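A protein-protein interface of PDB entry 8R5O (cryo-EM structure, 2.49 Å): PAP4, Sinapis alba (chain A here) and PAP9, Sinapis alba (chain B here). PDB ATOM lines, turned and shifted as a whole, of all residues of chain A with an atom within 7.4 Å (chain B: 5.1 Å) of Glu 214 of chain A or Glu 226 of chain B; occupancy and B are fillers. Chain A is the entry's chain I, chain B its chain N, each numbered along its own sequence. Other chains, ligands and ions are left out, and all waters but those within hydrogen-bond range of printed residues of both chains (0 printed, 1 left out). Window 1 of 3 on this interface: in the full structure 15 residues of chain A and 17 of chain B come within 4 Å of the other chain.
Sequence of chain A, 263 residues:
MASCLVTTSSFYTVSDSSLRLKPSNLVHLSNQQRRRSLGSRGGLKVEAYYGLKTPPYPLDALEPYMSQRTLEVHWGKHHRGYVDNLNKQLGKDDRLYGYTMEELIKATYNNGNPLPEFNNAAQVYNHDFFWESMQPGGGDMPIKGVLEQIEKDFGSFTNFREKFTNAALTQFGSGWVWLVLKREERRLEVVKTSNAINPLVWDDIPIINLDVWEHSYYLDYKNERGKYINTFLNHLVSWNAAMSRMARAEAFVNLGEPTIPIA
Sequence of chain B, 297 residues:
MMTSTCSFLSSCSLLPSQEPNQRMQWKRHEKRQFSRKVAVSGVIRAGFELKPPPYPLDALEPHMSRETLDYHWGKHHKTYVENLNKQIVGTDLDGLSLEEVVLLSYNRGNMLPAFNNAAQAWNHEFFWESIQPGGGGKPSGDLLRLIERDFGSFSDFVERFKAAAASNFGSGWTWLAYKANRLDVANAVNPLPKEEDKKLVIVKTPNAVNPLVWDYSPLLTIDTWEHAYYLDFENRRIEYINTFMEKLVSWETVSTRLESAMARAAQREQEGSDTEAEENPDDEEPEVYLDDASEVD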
ATOM      1  N   HIS A  78     -17.522  -5.316  23.115  1.00  0.00           N
ATOM      2  CA  HIS A  78     -16.243  -5.584  22.462  1.00  0.00           C
ATOM      3  C   HIS A  78     -15.094  -4.928  23.215  1.00  0.00           C
ATOM      4  O   HIS A  78     -14.140  -5.599  23.624  1.00  0.00           O
ATOM      5  CB  HIS A  78     -16.280  -5.102  21.011  1.00  0.00           C
ATOM      6  CG  HIS A  78     -17.114  -5.958  20.109  1.00  0.00           C
ATOM      7  ND1 HIS A  78     -16.686  -7.182  19.642  1.00  0.00           N
ATOM      8  CD2 HIS A  78     -18.345  -5.763  19.581  1.00  0.00           C
ATOM      9  CE1 HIS A  78     -17.619  -7.705  18.869  1.00  0.00           C
ATOM     10  NE2 HIS A  78     -18.636  -6.864  18.816  1.00  0.00           N
ATOM     11  N   TYR A  82     -12.127  -6.758  25.625  1.00  0.00           N
ATOM     12  CA  TYR A  82     -10.688  -6.610  25.437  1.00  0.00           C
ATOM     13  C   TYR A  82     -10.000  -6.188  26.728  1.00  0.00           C
ATOM     14  O   TYR A  82      -8.928  -6.701  27.065  1.00  0.00           O
ATOM     15  CB  TYR A  82     -10.408  -5.599  24.325  1.00  0.00           C
ATOM     16  CG  TYR A  82     -10.758  -6.087  22.941  1.00  0.00           C
ATOM     17  CD1 TYR A  82     -10.388  -7.354  22.517  1.00  0.00           C
ATOM     18  CD2 TYR A  82     -11.459  -5.280  22.059  1.00  0.00           C
ATOM     19  CE1 TYR A  82     -10.706  -7.802  21.250  1.00  0.00           C
ATOM     20  CE2 TYR A  82     -11.783  -5.720  20.794  1.00  0.00           C
ATOM     21  CZ  TYR A  82     -11.404  -6.979  20.393  1.00  0.00           C
ATOM     22  OH  TYR A  82     -11.727  -7.416  19.129  1.00  0.00           O
ATOM     23  N   GLY A 173     -11.053  -7.815   5.118  1.00  0.00           N
ATOM     24  CA  GLY A 173     -11.265  -8.378   6.433  1.00  0.00           C
ATOM     25  C   GLY A 173     -11.239  -7.318   7.520  1.00  0.00           C
ATOM     26  O   GLY A 173     -11.396  -6.118   7.276  1.00  0.00           O
ATOM     27  N   SER A 174     -11.039  -7.783   8.748  1.00  0.00           N
ATOM     28  CA  SER A 174     -10.971  -6.884   9.890  1.00  0.00           C
ATOM     29  C   SER A 174      -9.671  -6.090   9.869  1.00  0.00           C
ATOM     30  O   SER A 174      -8.623  -6.599   9.465  1.00  0.00           O
ATOM     31  CB  SER A 174     -11.079  -7.675  11.191  1.00  0.00           C
ATOM     32  OG  SER A 174     -12.287  -8.408  11.241  1.00  0.00           O
ATOM     33  N   GLY A 175      -9.740  -4.840  10.308  1.00  0.00           N
ATOM     34  CA  GLY A 175      -8.551  -4.017  10.343  1.00  0.00           C
ATOM     35  C   GLY A 175      -8.867  -2.596  10.762  1.00  0.00           C
ATOM     36  O   GLY A 175      -9.953  -2.298  11.261  1.00  0.00           O
ATOM     37  N   ASP A 211     -12.216   2.433  12.543  1.00  0.00           N
ATOM     38  CA  ASP A 211     -12.400   0.998  12.718  1.00  0.00           C
ATOM     39  C   ASP A 211     -13.180   0.441  11.533  1.00  0.00           C
ATOM     40  O   ASP A 211     -14.320   0.847  11.292  1.00  0.00           O
ATOM     41  CB  ASP A 211     -13.135   0.721  14.028  1.00  0.00           C
ATOM     42  CG  ASP A 211     -13.074  -0.736  14.439  1.00  0.00           C
ATOM     43  OD1 ASP A 211     -12.459  -1.541  13.715  1.00  0.00           O
ATOM     44  OD2 ASP A 211     -13.639  -1.076  15.498  1.00  0.00           O
ATOM     45  N   VAL A 212     -12.573  -0.485  10.797  1.00  0.00           N
ATOM     46  CA  VAL A 212     -13.263  -1.144   9.697  1.00  0.00           C
ATOM     47  C   VAL A 212     -13.503  -2.623   9.996  1.00  0.00           C
ATOM     48  O   VAL A 212     -13.765  -3.404   9.092  1.00  0.00           O
ATOM     49  CB  VAL A 212     -12.524  -0.945   8.358  1.00  0.00           C
ATOM     50  CG1 VAL A 212     -12.476   0.529   7.997  1.00  0.00           C
ATOM     51  CG2 VAL A 212     -11.128  -1.534   8.407  1.00  0.00           C
ATOM     52  N   TRP A 213     -13.410  -3.013  11.265  1.00  0.00           N
ATOM     53  CA  TRP A 213     -13.983  -4.282  11.688  1.00  0.00           C
ATOM     54  C   TRP A 213     -15.481  -4.261  11.422  1.00  0.00           C
ATOM     55  O   TRP A 213     -16.139  -3.231  11.591  1.00  0.00           O
ATOM     56  CB  TRP A 213     -13.718  -4.532  13.173  1.00  0.00           C
ATOM     57  CG  TRP A 213     -12.330  -4.984  13.501  1.00  0.00           C
ATOM     58  CD1 TRP A 213     -11.171  -4.308  13.268  1.00  0.00           C
ATOM     59  CD2 TRP A 213     -11.958  -6.203  14.154  1.00  0.00           C
ATOM     60  NE1 TRP A 213     -10.098  -5.036  13.718  1.00  0.00           N
ATOM     61  CE2 TRP A 213     -10.556  -6.204  14.269  1.00  0.00           C
ATOM     62  CE3 TRP A 213     -12.675  -7.298  14.643  1.00  0.00           C
ATOM     63  CZ2 TRP A 213      -9.856  -7.256  14.853  1.00  0.00           C
ATOM     64  CZ3 TRP A 213     -11.981  -8.338  15.224  1.00  0.00           C
ATOM     65  CH2 TRP A 213     -10.585  -8.310  15.326  1.00  0.00           C
ATOM     66  N   GLU A 214     -16.022  -5.401  10.994  1.00  0.00           N
ATOM     67  CA  GLU A 214     -17.428  -5.442  10.602  1.00  0.00           C
ATOM     68  C   GLU A 214     -18.355  -5.109  11.764  1.00  0.00           C
ATOM     69  O   GLU A 214     -19.447  -4.577  11.545  1.00  0.00           O
ATOM     70  CB  GLU A 214     -17.773  -6.807  10.011  1.00  0.00           C
ATOM     71  CG  GLU A 214     -17.378  -6.945   8.551  1.00  0.00           C
ATOM     72  CD  GLU A 214     -17.666  -8.321   7.983  1.00  0.00           C
ATOM     73  OE1 GLU A 214     -17.587  -9.308   8.741  1.00  0.00           O
ATOM     74  OE2 GLU A 214     -17.971  -8.412   6.776  1.00  0.00           O
ATOM     75  N   HIS A 215     -17.940  -5.390  13.002  1.00  0.00           N
ATOM     76  CA  HIS A 215     -18.806  -5.109  14.140  1.00  0.00           C
ATOM     77  C   HIS A 215     -19.019  -3.619  14.370  1.00  0.00           C
ATOM     78  O   HIS A 215     -19.930  -3.253  15.120  1.00  0.00           O
ATOM     79  CB  HIS A 215     -18.254  -5.761  15.415  1.00  0.00           C
ATOM     80  CG  HIS A 215     -16.933  -5.217  15.872  1.00  0.00           C
ATOM     81  ND1 HIS A 215     -15.816  -6.010  16.015  1.00  0.00           N
ATOM     82  CD2 HIS A 215     -16.559  -3.971  16.247  1.00  0.00           C
ATOM     83  CE1 HIS A 215     -14.807  -5.274  16.445  1.00  0.00           C
ATOM     84  NE2 HIS A 215     -15.231  -4.033  16.591  1.00  0.00           N
ATOM     85  N   SER A 216     -18.216  -2.757  13.752  1.00  0.00           N
ATOM     86  CA  SER A 216     -18.337  -1.319  13.952  1.00  0.00           C
ATOM     87  C   SER A 216     -19.379  -0.664  13.055  1.00  0.00           C
ATOM     88  O   SER A 216     -19.783   0.468  13.335  1.00  0.00           O
ATOM     89  CB  SER A 216     -16.982  -0.641  13.729  1.00  0.00           C
ATOM     90  OG  SER A 216     -16.531  -0.823  12.400  1.00  0.00           O
ATOM     91  N   TYR A 217     -19.828  -1.335  11.992  1.00  0.00           N
ATOM     92  CA  TYR A 217     -20.781  -0.720  11.080  1.00  0.00           C
ATOM     93  C   TYR A 217     -21.888  -1.642  10.586  1.00  0.00           C
ATOM     94  O   TYR A 217     -22.760  -1.174   9.848  1.00  0.00           O
ATOM     95  CB  TYR A 217     -20.050  -0.137   9.860  1.00  0.00           C
ATOM     96  CG  TYR A 217     -19.278  -1.151   9.044  1.00  0.00           C
ATOM     97  CD1 TYR A 217     -19.893  -1.866   8.024  1.00  0.00           C
ATOM     98  CD2 TYR A 217     -17.932  -1.383   9.283  1.00  0.00           C
ATOM     99  CE1 TYR A 217     -19.192  -2.790   7.277  1.00  0.00           C
ATOM    100  CE2 TYR A 217     -17.222  -2.303   8.538  1.00  0.00           C
ATOM    101  CZ  TYR A 217     -17.857  -3.005   7.536  1.00  0.00           C
ATOM    102  OH  TYR A 217     -17.157  -3.922   6.792  1.00  0.00           O
ATOM    103  N   TYR A 218     -21.895  -2.922  10.958  1.00  0.00           N
ATOM    104  CA  TYR A 218     -22.808  -3.851  10.302  1.00  0.00           C
ATOM    105  C   TYR A 218     -24.256  -3.640  10.726  1.00  0.00           C
ATOM    106  O   TYR A 218     -25.168  -3.895   9.936  1.00  0.00           O
ATOM    107  CB  TYR A 218     -22.387  -5.294  10.560  1.00  0.00           C
ATOM    108  CG  TYR A 218     -22.824  -6.225   9.458  1.00  0.00           C
ATOM    109  CD1 TYR A 218     -22.094  -6.324   8.283  1.00  0.00           C
ATOM    110  CD2 TYR A 218     -23.975  -6.989   9.579  1.00  0.00           C
ATOM    111  CE1 TYR A 218     -22.491  -7.159   7.266  1.00  0.00           C
ATOM    112  CE2 TYR A 218     -24.379  -7.831   8.567  1.00  0.00           C
ATOM    113  CZ  TYR A 218     -23.632  -7.913   7.412  1.00  0.00           C
ATOM    114  OH  TYR A 218     -24.026  -8.749   6.397  1.00  0.00           O
ATOM    115  N   LEU A 219     -24.493  -3.188  11.959  1.00  0.00           N
ATOM    116  CA  LEU A 219     -25.866  -2.943  12.386  1.00  0.00           C
ATOM    117  C   LEU A 219     -26.481  -1.757  11.653  1.00  0.00           C
ATOM    118  O   LEU A 219     -27.684  -1.761  11.369  1.00  0.00           O
ATOM    119  CB  LEU A 219     -25.926  -2.715  13.896  1.00  0.00           C
ATOM    120  CG  LEU A 219     -25.538  -3.899  14.782  1.00  0.00           C
ATOM    121  CD1 LEU A 219     -25.759  -3.567  16.250  1.00  0.00           C
ATOM    122  CD2 LEU A 219     -26.315  -5.144  14.387  1.00  0.00           C
ATOM    123  N   ASP A 220     -25.681  -0.738  11.343  1.00  0.00           N
ATOM    124  CA  ASP A 220     -26.195   0.477  10.728  1.00  0.00           C
ATOM    125  C   ASP A 220     -26.092   0.475   9.210  1.00  0.00           C
ATOM    126  O   ASP A 220     -26.890   1.145   8.545  1.00  0.00           O
ATOM    127  CB  ASP A 220     -25.452   1.697  11.278  1.00  0.00           C
ATOM    128  CG  ASP A 220     -25.593   1.836  12.779  1.00  0.00           C
ATOM    129  OD1 ASP A 220     -26.659   1.467  13.314  1.00  0.00           O
ATOM    130  OD2 ASP A 220     -24.638   2.316  13.422  1.00  0.00           O
ATOM    131  N   LYS A 222     -24.744  -2.662   7.285  1.00  0.00           N
ATOM    132  CA  LYS A 222     -24.641  -4.021   6.741  1.00  0.00           C
ATOM    133  C   LYS A 222     -23.381  -4.098   5.886  1.00  0.00           C
ATOM    134  O   LYS A 222     -22.290  -3.807   6.403  1.00  0.00           O
ATOM    135  CB  LYS A 222     -25.948  -4.386   6.031  1.00  0.00           C
ATOM    136  CG  LYS A 222     -26.997  -5.025   6.925  1.00  0.00           C
ATOM    137  CD  LYS A 222     -27.622  -4.023   7.874  1.00  0.00           C
ATOM    138  CE  LYS A 222     -28.592  -4.700   8.822  1.00  0.00           C
ATOM    139  NZ  LYS A 222     -29.112  -3.755   9.845  1.00  0.00           N
ATOM    140  N   ASN A 223     -23.467  -4.468   4.609  1.00  0.00           N
ATOM    141  CA  ASN A 223     -22.299  -4.628   3.753  1.00  0.00           C
ATOM    142  C   ASN A 223     -21.818  -3.317   3.146  1.00  0.00           C
ATOM    143  O   ASN A 223     -20.783  -3.312   2.471  1.00  0.00           O
ATOM    144  CB  ASN A 223     -22.611  -5.622   2.633  1.00  0.00           C
ATOM    145  CG  ASN A 223     -23.735  -5.146   1.734  1.00  0.00           C
ATOM    146  OD1 ASN A 223     -24.901  -5.161   2.121  1.00  0.00           O
ATOM    147  ND2 ASN A 223     -23.388  -4.721   0.525  1.00  0.00           N
ATOM    148  N   ARG A 225     -19.898  -0.743   3.495  1.00  0.00           N
ATOM    149  CA  ARG A 225     -18.779  -0.097   4.172  1.00  0.00           C
ATOM    150  C   ARG A 225     -18.506   1.284   3.596  1.00  0.00           C
ATOM    151  O   ARG A 225     -18.090   2.188   4.328  1.00  0.00           O
ATOM    152  CB  ARG A 225     -17.524  -0.966   4.083  1.00  0.00           C
ATOM    153  CG  ARG A 225     -16.383  -0.458   4.948  1.00  0.00           C
ATOM    154  CD  ARG A 225     -15.053  -1.087   4.587  1.00  0.00           C
ATOM    155  NE  ARG A 225     -14.911  -2.440   5.104  1.00  0.00           N
ATOM    156  CZ  ARG A 225     -13.778  -3.128   5.088  1.00  0.00           C
ATOM    157  NH1 ARG A 225     -12.667  -2.616   4.587  1.00  0.00           N
ATOM    158  NH2 ARG A 225     -13.758  -4.358   5.593  1.00  0.00           N
ATOM    159  N   HIS B  76     -23.050 -10.669   0.319  1.00  0.00           N
ATOM    160  CA  HIS B  76     -21.628 -10.969   0.450  1.00  0.00           C
ATOM    161  C   HIS B  76     -21.187 -12.011  -0.570  1.00  0.00           C
ATOM    162  O   HIS B  76     -20.246 -11.786  -1.340  1.00  0.00           O
ATOM    163  CB  HIS B  76     -21.319 -11.440   1.871  1.00  0.00           C
ATOM    164  CG  HIS B  76     -21.485 -10.377   2.911  1.00  0.00           C
ATOM    165  ND1 HIS B  76     -20.503  -9.454   3.193  1.00  0.00           N
ATOM    166  CD2 HIS B  76     -22.517 -10.091   3.738  1.00  0.00           C
ATOM    167  CE1 HIS B  76     -20.923  -8.645   4.147  1.00  0.00           C
ATOM    168  NE2 HIS B  76     -22.142  -9.011   4.496  1.00  0.00           N
ATOM    169  N   SER B 171     -11.368 -12.087  11.185  1.00  0.00           N
ATOM    170  CA  SER B 171     -12.129 -12.820  10.186  1.00  0.00           C
ATOM    171  C   SER B 171     -11.373 -14.073   9.764  1.00  0.00           C
ATOM    172  O   SER B 171     -10.155 -14.043   9.571  1.00  0.00           O
ATOM    173  CB  SER B 171     -12.395 -11.937   8.967  1.00  0.00           C
ATOM    174  OG  SER B 171     -13.071 -10.749   9.330  1.00  0.00           O
ATOM    175  N   THR B 224     -16.488 -17.788  10.466  1.00  0.00           N
ATOM    176  CA  THR B 224     -16.322 -16.958  11.652  1.00  0.00           C
ATOM    177  C   THR B 224     -16.114 -15.489  11.312  1.00  0.00           C
ATOM    178  O   THR B 224     -15.740 -14.709  12.194  1.00  0.00           O
ATOM    179  CB  THR B 224     -15.165 -17.469  12.514  1.00  0.00           C
ATOM    180  OG1 THR B 224     -14.055 -17.822  11.681  1.00  0.00           O
ATOM    181  CG2 THR B 224     -15.600 -18.683  13.321  1.00  0.00           C
ATOM    182  N   TRP B 225     -16.338 -15.092  10.062  1.00  0.00           N
ATOM    183  CA  TRP B 225     -16.494 -13.678   9.761  1.00  0.00           C
ATOM    184  C   TRP B 225     -17.699 -13.145  10.523  1.00  0.00           C
ATOM    185  O   TRP B 225     -18.711 -13.834  10.672  1.00  0.00           O
ATOM    186  CB  TRP B 225     -16.680 -13.455   8.259  1.00  0.00           C
ATOM    187  CG  TRP B 225     -15.433 -13.617   7.433  1.00  0.00           C
ATOM    188  CD1 TRP B 225     -14.668 -14.737   7.312  1.00  0.00           C
ATOM    189  CD2 TRP B 225     -14.835 -12.630   6.586  1.00  0.00           C
ATOM    190  NE1 TRP B 225     -13.622 -14.507   6.456  1.00  0.00           N
ATOM    191  CE2 TRP B 225     -13.700 -13.220   5.995  1.00  0.00           C
ATOM    192  CE3 TRP B 225     -15.141 -11.302   6.276  1.00  0.00           C
ATOM    193  CZ2 TRP B 225     -12.874 -12.529   5.113  1.00  0.00           C
ATOM    194  CZ3 TRP B 225     -14.321 -10.619   5.402  1.00  0.00           C
ATOM    195  CH2 TRP B 225     -13.200 -11.232   4.830  1.00  0.00           C
ATOM    196  N   GLU B 226     -17.585 -11.913  11.020  1.00  0.00           N
ATOM    197  CA  GLU B 226     -18.630 -11.379  11.884  1.00  0.00           C
ATOM    198  C   GLU B 226     -19.958 -11.220  11.151  1.00  0.00           C
ATOM    199  O   GLU B 226     -21.018 -11.287  11.781  1.00  0.00           O
ATOM    200  CB  GLU B 226     -18.178 -10.052  12.492  1.00  0.00           C
ATOM    201  CG  GLU B 226     -17.132 -10.228  13.582  1.00  0.00           C
ATOM    202  CD  GLU B 226     -16.609  -8.915  14.127  1.00  0.00           C
ATOM    203  OE1 GLU B 226     -16.456  -7.958  13.342  1.00  0.00           O
ATOM    204  OE2 GLU B 226     -16.350  -8.844  15.346  1.00  0.00           O
ATOM    205  N   HIS B 227     -19.930 -11.032   9.830  1.00  0.00           N
ATOM    206  CA  HIS B 227     -21.178 -10.903   9.084  1.00  0.00           C
ATOM    207  C   HIS B 227     -21.994 -12.189   9.081  1.00  0.00           C
ATOM    208  O   HIS B 227     -23.188 -12.150   8.776  1.00  0.00           O
ATOM    209  CB  HIS B 227     -20.906 -10.454   7.645  1.00  0.00           C
ATOM    210  CG  HIS B 227     -20.121 -11.436   6.826  1.00  0.00           C
ATOM    211  ND1 HIS B 227     -18.899 -11.126   6.269  1.00  0.00           N
ATOM    212  CD2 HIS B 227     -20.392 -12.707   6.450  1.00  0.00           C
ATOM    213  CE1 HIS B 227     -18.447 -12.167   5.597  1.00  0.00           C
ATOM    214  NE2 HIS B 227     -19.332 -13.141   5.693  1.00  0.00           N
ATOM    215  N   ALA B 228     -21.378 -13.326   9.410  1.00  0.00           N
ATOM    216  CA  ALA B 228     -22.095 -14.595   9.398  1.00  0.00           C
ATOM    217  C   ALA B 228     -23.030 -14.755  10.589  1.00  0.00           C
ATOM    218  O   ALA B 228     -23.976 -15.543  10.510  1.00  0.00           O
ATOM    219  CB  ALA B 228     -21.101 -15.756   9.360  1.00  0.00           C
ATOM    220  N   TYR B 229     -22.794 -14.035  11.687  1.00  0.00           N
ATOM    221  CA  TYR B 229     -23.590 -14.234  12.889  1.00  0.00           C
ATOM    222  C   TYR B 229     -24.000 -12.955  13.605  1.00  0.00           C
ATOM    223  O   TYR B 229     -24.718 -13.045  14.604  1.00  0.00           O
ATOM    224  CB  TYR B 229     -22.832 -15.131  13.883  1.00  0.00           C
ATOM    225  CG  TYR B 229     -21.510 -14.561  14.354  1.00  0.00           C
ATOM    226  CD1 TYR B 229     -21.443 -13.737  15.470  1.00  0.00           C
ATOM    227  CD2 TYR B 229     -20.330 -14.856  13.690  1.00  0.00           C
ATOM    228  CE1 TYR B 229     -20.239 -13.216  15.903  1.00  0.00           C
ATOM    229  CE2 TYR B 229     -19.123 -14.343  14.117  1.00  0.00           C
ATOM    230  CZ  TYR B 229     -19.083 -13.523  15.224  1.00  0.00           C
ATOM    231  OH  TYR B 229     -17.881 -13.011  15.651  1.00  0.00           O
ATOM    232  N   TYR B 230     -23.579 -11.777  13.144  1.00  0.00           N
ATOM    233  CA  TYR B 230     -23.791 -10.574  13.942  1.00  0.00           C
ATOM    234  C   TYR B 230     -25.256 -10.166  13.993  1.00  0.00           C
ATOM    235  O   TYR B 230     -25.699  -9.583  14.989  1.00  0.00           O
ATOM    236  CB  TYR B 230     -22.939  -9.422  13.414  1.00  0.00           C
ATOM    237  CG  TYR B 230     -22.375  -8.567  14.521  1.00  0.00           C
ATOM    238  CD1 TYR B 230     -21.283  -8.995  15.260  1.00  0.00           C
ATOM    239  CD2 TYR B 230     -22.944  -7.344  14.841  1.00  0.00           C
ATOM    240  CE1 TYR B 230     -20.768  -8.228  16.281  1.00  0.00           C
ATOM    241  CE2 TYR B 230     -22.434  -6.566  15.859  1.00  0.00           C
ATOM    242  CZ  TYR B 230     -21.346  -7.014  16.576  1.00  0.00           C
ATOM    243  OH  TYR B 230     -20.829  -6.246  17.592  1.00  0.00           O
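The side-chain carboxylate (OE1) of Glu 214 of chain A lies within hydrogen-bond range of the backbone NH (N) of Glu 226 of chain B (3.5 Å).
The side-chain hydroxyl (OH) of Tyr 230 of chain B lies within hydrogen-bond range of a ring nitrogen (NE2) of His 78 of chain A.
ND1 of His 227 of chain B sits at hydrogen-bond distance from OE2 of Glu 214 of chain A (2.9 Å).
A ring nitrogen (ND1) of His 215 of chain A lies within hydrogen-bond range of the side-chain carboxylate (OE2) of Glu 226 of chain B, 3.0 Å away.
OG of Ser 174 of chain A sits at hydrogen-bond distance from OG of Ser 171 of chain B (3.1 Å).
NE2 of His 76 of chain B is in hydrogen-bond range of OH of Tyr 218 of chain A (2.7 Å).
Hydrophobic or aromatic side chains of chain A that line the printed part of chain B: His 78, His 215 and Tyr 218.
Of the 9 printed residues of chain B, 6 touch a printed residue of chain A.
Hydrophobic or aromatic side chains of chain B that line the printed part of chain A: His 76, Trp 225, His 227 and Tyr 230.
Among the printed residues, 12 pairs touch across the chains.
Among the printed residues, no Asp or Glu carboxylate lies within 4 Å of a Lys or Arg side-chain nitrogen of the other chain.
Among the printed residues, pairs that only touch across the chains: His 215 of chain A with Tyr 230 of chain B (3.4 Å), Tyr 218 of chain A with His 227 of chain B (3.7 Å), Asn 223 of chain A with His 76 of chain B (3.8 Å), Gly 173 of chain A with Trp 225 of chain B (3.8 Å), His 78 of chain A with Glu 226 of chain B (3.9 Å) and Glu 214 of chain A with His 76 of chain B (3.96 Å).
Of the printed residues of chain B, Glu 214 of chain A touches His 76, Glu 226 and His 227.
Of chain A, only His 78 (3.9 Å), Glu 214 (3.5 Å) and His 215 (3.0 Å) come within 4 Å of Glu 226 of chain B.
Printed residues of chain B within 4 Å of Tyr 218 of chain A: His 76 and His 227.
Of the printed residues of chain A, His 227 of chain B touches Glu 214 (2.9 Å) and Tyr 218 (3.7 Å).
Of the printed residues of chain A, Trp 225 of chain B touches Gly 173 (3.8 Å).
Ala 228 of chain B touches none of the printed residues of chain A.
Asp 220 of chain A touches none of the printed residues of chain B.
O of Gly 173 of chain A sits at hydrogen-bond distance from NH2 of Arg 225 of chain A (3.4 Å).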
